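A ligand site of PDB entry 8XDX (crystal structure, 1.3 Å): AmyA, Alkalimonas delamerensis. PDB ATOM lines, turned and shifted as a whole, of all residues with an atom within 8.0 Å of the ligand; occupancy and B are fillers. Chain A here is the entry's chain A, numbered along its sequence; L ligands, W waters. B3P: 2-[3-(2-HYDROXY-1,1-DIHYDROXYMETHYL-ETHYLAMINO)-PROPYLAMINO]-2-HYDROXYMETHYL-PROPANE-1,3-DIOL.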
ATOM      1  N   THR A 173      -6.954  11.230  22.240  1.00  0.00           N
ATOM      2  CA  THR A 173      -7.612  12.119  23.190  1.00  0.00           C
ATOM      3  C   THR A 173      -8.249  11.314  24.310  1.00  0.00           C
ATOM      4  O   THR A 173      -8.538  10.124  24.159  1.00  0.00           O
ATOM      5  CB  THR A 173      -8.726  12.921  22.500  1.00  0.00           C
ATOM      6  OG1 THR A 173      -9.763  12.027  22.088  1.00  0.00           O
ATOM      7  CG2 THR A 173      -8.204  13.715  21.308  1.00  0.00           C
ATOM      8  N   GLN A 174      -8.490  11.987  25.440  1.00  0.00           N
ATOM      9  CA  GLN A 174      -9.211  11.329  26.529  1.00  0.00           C
ATOM     10  C   GLN A 174     -10.657  11.033  26.146  1.00  0.00           C
ATOM     11  O   GLN A 174     -11.209  10.001  26.545  1.00  0.00           O
ATOM     12  CB  GLN A 174      -9.144  12.198  27.793  1.00  0.00           C
ATOM     13  CG  GLN A 174      -9.748  11.556  29.036  1.00  0.00           C
ATOM     14  CD  GLN A 174      -9.626  12.439  30.277  1.00  0.00           C
ATOM     15  OE1 GLN A 174      -9.473  13.660  30.162  1.00  0.00           O
ATOM     16  NE2 GLN A 174      -9.688  11.823  31.460  1.00  0.00           N
ATOM     17  N   GLN A 175     -11.266  11.910  25.351  1.00  0.00           N
ATOM     18  CA  GLN A 175     -12.630  11.672  24.870  1.00  0.00           C
ATOM     19  C   GLN A 175     -12.735  10.323  24.159  1.00  0.00           C
ATOM     20  O   GLN A 175     -13.729   9.612  24.313  1.00  0.00           O
ATOM     21  CB  GLN A 175     -13.048  12.833  23.954  1.00  0.00           C
ATOM     22  CG  GLN A 175     -14.234  12.562  23.038  1.00  0.00           C
ATOM     23  CD  GLN A 175     -15.570  12.520  23.756  1.00  0.00           C
ATOM     24  OE1 GLN A 175     -15.646  12.704  24.978  1.00  0.00           O
ATOM     25  NE2 GLN A 175     -16.627  12.209  23.016  1.00  0.00           N
ATOM     26  N   ASN A 176     -11.701   9.955  23.401  1.00  0.00           N
ATOM     27  CA  ASN A 176     -11.725   8.664  22.704  1.00  0.00           C
ATOM     28  C   ASN A 176     -11.307   7.510  23.605  1.00  0.00           C
ATOM     29  O   ASN A 176     -11.939   6.448  23.577  1.00  0.00           O
ATOM     30  CB  ASN A 176     -10.811   8.696  21.479  1.00  0.00           C
ATOM     31  CG  ASN A 176     -11.452   9.398  20.309  1.00  0.00           C
ATOM     32  OD1 ASN A 176     -12.681   9.463  20.197  1.00  0.00           O
ATOM     33  ND2 ASN A 176     -10.624   9.922  19.407  1.00  0.00           N
ATOM     34  N   TRP A 177     -10.255   7.681  24.407  1.00  0.00           N
ATOM     35  CA  TRP A 177      -9.540   6.542  24.983  1.00  0.00           C
ATOM     36  C   TRP A 177      -9.560   6.448  26.494  1.00  0.00           C
ATOM     37  O   TRP A 177      -8.984   5.490  27.037  1.00  0.00           O
ATOM     38  CB  TRP A 177      -8.090   6.487  24.455  1.00  0.00           C
ATOM     39  CG  TRP A 177      -8.061   6.616  22.971  1.00  0.00           C
ATOM     40  CD1 TRP A 177      -7.533   7.636  22.243  1.00  0.00           C
ATOM     41  CD2 TRP A 177      -8.635   5.705  22.029  1.00  0.00           C
ATOM     42  NE1 TRP A 177      -7.740   7.415  20.902  1.00  0.00           N
ATOM     43  CE2 TRP A 177      -8.417   6.239  20.746  1.00  0.00           C
ATOM     44  CE3 TRP A 177      -9.331   4.499  22.160  1.00  0.00           C
ATOM     45  CZ2 TRP A 177      -8.865   5.603  19.596  1.00  0.00           C
ATOM     46  CZ3 TRP A 177      -9.763   3.860  21.016  1.00  0.00           C
ATOM     47  CH2 TRP A 177      -9.540   4.425  19.751  1.00  0.00           C
ATOM     48  N   GLY A 178     -10.207   7.385  27.190  1.00  0.00           N
ATOM     49  CA  GLY A 178     -10.299   7.288  28.641  1.00  0.00           C
ATOM     50  C   GLY A 178      -8.934   7.186  29.284  1.00  0.00           C
ATOM     51  O   GLY A 178      -8.019   7.954  28.982  1.00  0.00           O
ATOM     52  N   TYR A 179      -8.780   6.188  30.155  1.00  0.00           N
ATOM     53  CA  TYR A 179      -7.560   6.093  30.970  1.00  0.00           C
ATOM     54  C   TYR A 179      -6.307   5.814  30.151  1.00  0.00           C
ATOM     55  O   TYR A 179      -5.203   6.016  30.663  1.00  0.00           O
ATOM     56  CB  TYR A 179      -7.723   5.059  32.087  1.00  0.00           C
ATOM     57  CG  TYR A 179      -7.323   3.642  31.706  1.00  0.00           C
ATOM     58  CD1 TYR A 179      -8.139   2.831  30.925  1.00  0.00           C
ATOM     59  CD2 TYR A 179      -6.115   3.102  32.149  1.00  0.00           C
ATOM     60  CE1 TYR A 179      -7.774   1.531  30.601  1.00  0.00           C
ATOM     61  CE2 TYR A 179      -5.741   1.810  31.842  1.00  0.00           C
ATOM     62  CZ  TYR A 179      -6.568   1.026  31.053  1.00  0.00           C
ATOM     63  OH  TYR A 179      -6.190  -0.262  30.753  1.00  0.00           O
ATOM     64  N   LEU A 180      -6.444   5.347  28.901  1.00  0.00           N
ATOM     65  CA  LEU A 180      -5.268   5.142  28.059  1.00  0.00           C
ATOM     66  C   LEU A 180      -4.654   6.440  27.576  1.00  0.00           C
ATOM     67  O   LEU A 180      -3.525   6.420  27.061  1.00  0.00           O
ATOM     68  CB  LEU A 180      -5.627   4.269  26.862  1.00  0.00           C
ATOM     69  CG  LEU A 180      -6.057   2.838  27.156  1.00  0.00           C
ATOM     70  CD1 LEU A 180      -6.393   2.114  25.870  1.00  0.00           C
ATOM     71  CD2 LEU A 180      -4.987   2.084  27.944  1.00  0.00           C
ATOM     72  N   TRP A 181      -5.341   7.573  27.733  1.00  0.00           N
ATOM     73  CA  TRP A 181      -4.803   8.850  27.276  1.00  0.00           C
ATOM     74  C   TRP A 181      -3.885   9.461  28.330  1.00  0.00           C
ATOM     75  O   TRP A 181      -4.233   9.529  29.518  1.00  0.00           O
ATOM     76  CB  TRP A 181      -5.925   9.825  26.935  1.00  0.00           C
ATOM     77  CG  TRP A 181      -5.357  11.103  26.411  1.00  0.00           C
ATOM     78  CD1 TRP A 181      -4.867  11.328  25.159  1.00  0.00           C
ATOM     79  CD2 TRP A 181      -5.193  12.335  27.140  1.00  0.00           C
ATOM     80  NE1 TRP A 181      -4.408  12.619  25.058  1.00  0.00           N
ATOM     81  CE2 TRP A 181      -4.599  13.254  26.256  1.00  0.00           C
ATOM     82  CE3 TRP A 181      -5.490  12.737  28.439  1.00  0.00           C
ATOM     83  CZ2 TRP A 181      -4.302  14.574  26.634  1.00  0.00           C
ATOM     84  CZ3 TRP A 181      -5.193  14.044  28.812  1.00  0.00           C
ATOM     85  CH2 TRP A 181      -4.613  14.944  27.920  1.00  0.00           C
ATOM     86  N   LYS A 230      -1.525   0.990  22.935  1.00  0.00           N
ATOM     87  CA  LYS A 230      -2.742   0.219  23.173  1.00  0.00           C
ATOM     88  C   LYS A 230      -3.950   0.915  22.587  1.00  0.00           C
ATOM     89  O   LYS A 230      -4.790   0.288  21.922  1.00  0.00           O
ATOM     90  CB  LYS A 230      -2.933  -0.027  24.666  1.00  0.00           C
ATOM     91  CG  LYS A 230      -1.921  -0.990  25.257  1.00  0.00           C
ATOM     92  CD  LYS A 230      -2.074  -1.185  26.753  1.00  0.00           C
ATOM     93  CE  LYS A 230      -0.887  -1.983  27.292  1.00  0.00           C
ATOM     94  NZ  LYS A 230      -0.804  -2.006  28.761  1.00  0.00           N
ATOM     95  N   ALA A 231      -4.059   2.228  22.808  1.00  0.00           N
ATOM     96  CA  ALA A 231      -5.170   2.980  22.241  1.00  0.00           C
ATOM     97  C   ALA A 231      -5.120   2.961  20.724  1.00  0.00           C
ATOM     98  O   ALA A 231      -6.154   2.785  20.063  1.00  0.00           O
ATOM     99  CB  ALA A 231      -5.133   4.419  22.755  1.00  0.00           C
ATOM    100  N   GLU A 234      -6.453  -0.369  19.333  1.00  0.00           N
ATOM    101  CA  GLU A 234      -7.918  -0.364  19.361  1.00  0.00           C
ATOM    102  C   GLU A 234      -8.468   0.499  18.234  1.00  0.00           C
ATOM    103  O   GLU A 234      -9.465   0.131  17.592  1.00  0.00           O
ATOM    104  CB  GLU A 234      -8.416   0.174  20.707  1.00  0.00           C
ATOM    105  CG  GLU A 234      -8.218  -0.757  21.880  1.00  0.00           C
ATOM    106  CD  GLU A 234      -8.922  -0.274  23.126  1.00  0.00           C
ATOM    107  OE1 GLU A 234      -8.338  -0.386  24.219  1.00  0.00           O
ATOM    108  OE2 GLU A 234     -10.069   0.207  22.991  1.00  0.00           O
ATOM    109  N   TRP A 235      -7.847   1.649  17.985  1.00  0.00           N
ATOM    110  CA  TRP A 235      -8.307   2.532  16.912  1.00  0.00           C
ATOM    111  C   TRP A 235      -8.256   1.827  15.563  1.00  0.00           C
ATOM    112  O   TRP A 235      -9.219   1.858  14.795  1.00  0.00           O
ATOM    113  CB  TRP A 235      -7.427   3.773  16.915  1.00  0.00           C
ATOM    114  CG  TRP A 235      -7.808   4.837  15.931  1.00  0.00           C
ATOM    115  CD1 TRP A 235      -8.980   5.556  15.909  1.00  0.00           C
ATOM    116  CD2 TRP A 235      -6.999   5.353  14.882  1.00  0.00           C
ATOM    117  NE1 TRP A 235      -8.940   6.470  14.882  1.00  0.00           N
ATOM    118  CE2 TRP A 235      -7.737   6.357  14.227  1.00  0.00           C
ATOM    119  CE3 TRP A 235      -5.717   5.034  14.404  1.00  0.00           C
ATOM    120  CZ2 TRP A 235      -7.230   7.065  13.137  1.00  0.00           C
ATOM    121  CZ3 TRP A 235      -5.215   5.719  13.317  1.00  0.00           C
ATOM    122  CH2 TRP A 235      -5.970   6.727  12.693  1.00  0.00           C
ATOM    123  N   ASN A 238     -11.007  -1.268  15.806  1.00  0.00           N
ATOM    124  CA  ASN A 238     -12.398  -0.983  16.136  1.00  0.00           C
ATOM    125  C   ASN A 238     -12.929   0.279  15.474  1.00  0.00           C
ATOM    126  O   ASN A 238     -14.138   0.386  15.255  1.00  0.00           O
ATOM    127  CB  ASN A 238     -12.581  -0.876  17.640  1.00  0.00           C
ATOM    128  CG  ASN A 238     -12.460  -2.199  18.336  1.00  0.00           C
ATOM    129  OD1 ASN A 238     -12.688  -3.249  17.732  1.00  0.00           O
ATOM    130  ND2 ASN A 238     -12.100  -2.160  19.616  1.00  0.00           N
ATOM    131  N   HIS A 264      -3.479  -7.024  24.873  1.00  0.00           N
ATOM    132  CA  HIS A 264      -4.457  -5.956  25.079  1.00  0.00           C
ATOM    133  C   HIS A 264      -5.387  -5.842  23.891  1.00  0.00           C
ATOM    134  O   HIS A 264      -6.619  -5.811  24.034  1.00  0.00           O
ATOM    135  CB  HIS A 264      -3.759  -4.611  25.284  1.00  0.00           C
ATOM    136  CG  HIS A 264      -4.744  -3.484  25.364  1.00  0.00           C
ATOM    137  ND1 HIS A 264      -5.313  -3.091  26.549  1.00  0.00           N
ATOM    138  CD2 HIS A 264      -5.316  -2.724  24.400  1.00  0.00           C
ATOM    139  CE1 HIS A 264      -6.180  -2.124  26.327  1.00  0.00           C
ATOM    140  NE2 HIS A 264      -6.200  -1.878  25.031  1.00  0.00           N
ATOM    141  N   TRP A 267      -7.928  -8.650  23.430  1.00  0.00           N
ATOM    142  CA  TRP A 267      -9.034  -8.679  24.369  1.00  0.00           C
ATOM    143  C   TRP A 267      -9.966  -7.469  24.254  1.00  0.00           C
ATOM    144  O   TRP A 267     -11.102  -7.532  24.692  1.00  0.00           O
ATOM    145  CB  TRP A 267      -8.516  -8.974  25.778  1.00  0.00           C
ATOM    146  CG  TRP A 267      -8.155 -10.450  25.832  1.00  0.00           C
ATOM    147  CD1 TRP A 267      -6.945 -11.029  25.538  1.00  0.00           C
ATOM    148  CD2 TRP A 267      -9.048 -11.542  26.105  1.00  0.00           C
ATOM    149  NE1 TRP A 267      -7.025 -12.390  25.651  1.00  0.00           N
ATOM    150  CE2 TRP A 267      -8.307 -12.728  25.998  1.00  0.00           C
ATOM    151  CE3 TRP A 267     -10.395 -11.616  26.449  1.00  0.00           C
ATOM    152  CZ2 TRP A 267      -8.865 -13.986  26.220  1.00  0.00           C
ATOM    153  CZ3 TRP A 267     -10.953 -12.861  26.676  1.00  0.00           C
ATOM    154  CH2 TRP A 267     -10.194 -14.030  26.564  1.00  0.00           C
ATOM    155  N   ALA A 268      -9.502  -6.404  23.610  1.00  0.00           N
ATOM    156  CA  ALA A 268     -10.332  -5.216  23.403  1.00  0.00           C
ATOM    157  C   ALA A 268     -11.117  -5.258  22.109  1.00  0.00           C
ATOM    158  O   ALA A 268     -11.778  -4.296  21.757  1.00  0.00           O
ATOM    159  CB  ALA A 268      -9.432  -3.994  23.393  1.00  0.00           C
HETATM  160  C1  B3P L   1     -13.829   4.380  27.097  1.00  0.00           C
HETATM  161  C2  B3P L   1     -13.925   5.896  27.020  1.00  0.00           C
HETATM  162  C3  B3P L   1     -12.405   3.947  26.753  1.00  0.00           C
HETATM  163  N1  B3P L   1     -12.260   2.502  26.816  1.00  0.00           N
HETATM  164  C4  B3P L   1     -10.922   1.938  26.733  1.00  0.00           C
HETATM  165  C5  B3P L   1     -11.041   0.412  26.654  1.00  0.00           C
HETATM  166  C6  B3P L   1     -10.184   2.512  25.531  1.00  0.00           C
HETATM  167  C7  B3P L   1     -10.147   2.332  27.986  1.00  0.00           C
HETATM  168  N2  B3P L   1     -15.104   6.414  27.689  1.00  0.00           N
HETATM  169  C8  B3P L   1     -15.434   7.817  27.508  1.00  0.00           C
HETATM  170  C9  B3P L   1     -16.479   8.231  28.532  1.00  0.00           C
HETATM  171  C10 B3P L   1     -15.976   8.005  26.104  1.00  0.00           C
HETATM  172  C11 B3P L   1     -14.173   8.654  27.707  1.00  0.00           C
HETATM  173  O1  B3P L   1     -17.641   7.414  28.345  1.00  0.00           O
HETATM  174  O2  B3P L   1     -16.161   9.407  25.848  1.00  0.00           O
HETATM  175  O3  B3P L   1     -13.605   8.335  28.978  1.00  0.00           O
HETATM  176  O4  B3P L   1      -9.749  -0.184  26.562  1.00  0.00           O
HETATM  177  O5  B3P L   1     -10.943   2.270  24.351  1.00  0.00           O
HETATM  178  O6  B3P L   1     -10.955   2.086  29.143  1.00  0.00           O
HETATM  179  O   HOH W   1     -13.919  11.037  30.498  1.00  0.00           O
HETATM  180  O   HOH W   2     -13.699   2.783  31.056  1.00  0.00           O
HETATM  181  O   HOH W   3     -10.838  -0.401  30.344  1.00  0.00           O
HETATM  182  O   HOH W   4     -11.238   4.700  30.915  1.00  0.00           O
HETATM  183  O   HOH W   5     -14.114   1.180  25.129  1.00  0.00           O
HETATM  184  O   HOH W   6      -7.989  -1.387  28.948  1.00  0.00           O
HETATM  185  O   HOH W   7     -17.077   4.682  26.735  1.00  0.00           O
HETATM  186  O   HOH W   8     -10.073  -3.130  26.779  1.00  0.00           O
HETATM  187  O   HOH W   9     -12.757   3.876  23.176  1.00  0.00           O
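The side-chain amide oxygen (OE1) of Gln 175 lies within hydrogen-bond range of an oxygen (O2) of the ligand, at 3.4 Å. The side-chain carboxylate of Glu 234 is in hydrogen-bond range of an oxygen (O5) of the ligand. O of Gln 175 is in hydrogen-bond range of O2 of the ligand (2.9 Å).
OE1 of Glu 234 lies within hydrogen-bond range of NE2 of His 264.
Merely in contact with the ligand: Gln 174 (3.5 Å), Trp 177 (3.5 Å), Gly 178 (3.5 Å), Tyr 179 (3.4 Å) and Leu 180 (3.8 Å). Hydrophobic or aromatic side chains that line the ligand: Trp 177, Tyr 179 and Leu 180. Within 4 Å of the ligand: Gln 174, Gln 175, Trp 177, Gly 178, Tyr 179, Leu 180 and Glu 234.
Water W9 lies within hydrogen-bond range of an oxygen (O5) of the ligand and the backbone carbonyl oxygen of Asn 176. Water W4 lies within hydrogen-bond range of N of Tyr 179 (3.0 Å) and O6 of the ligand (3.2 Å). Water W6 bridges the side-chain hydroxyl of Tyr 179 and an oxygen (O4) of the ligand.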
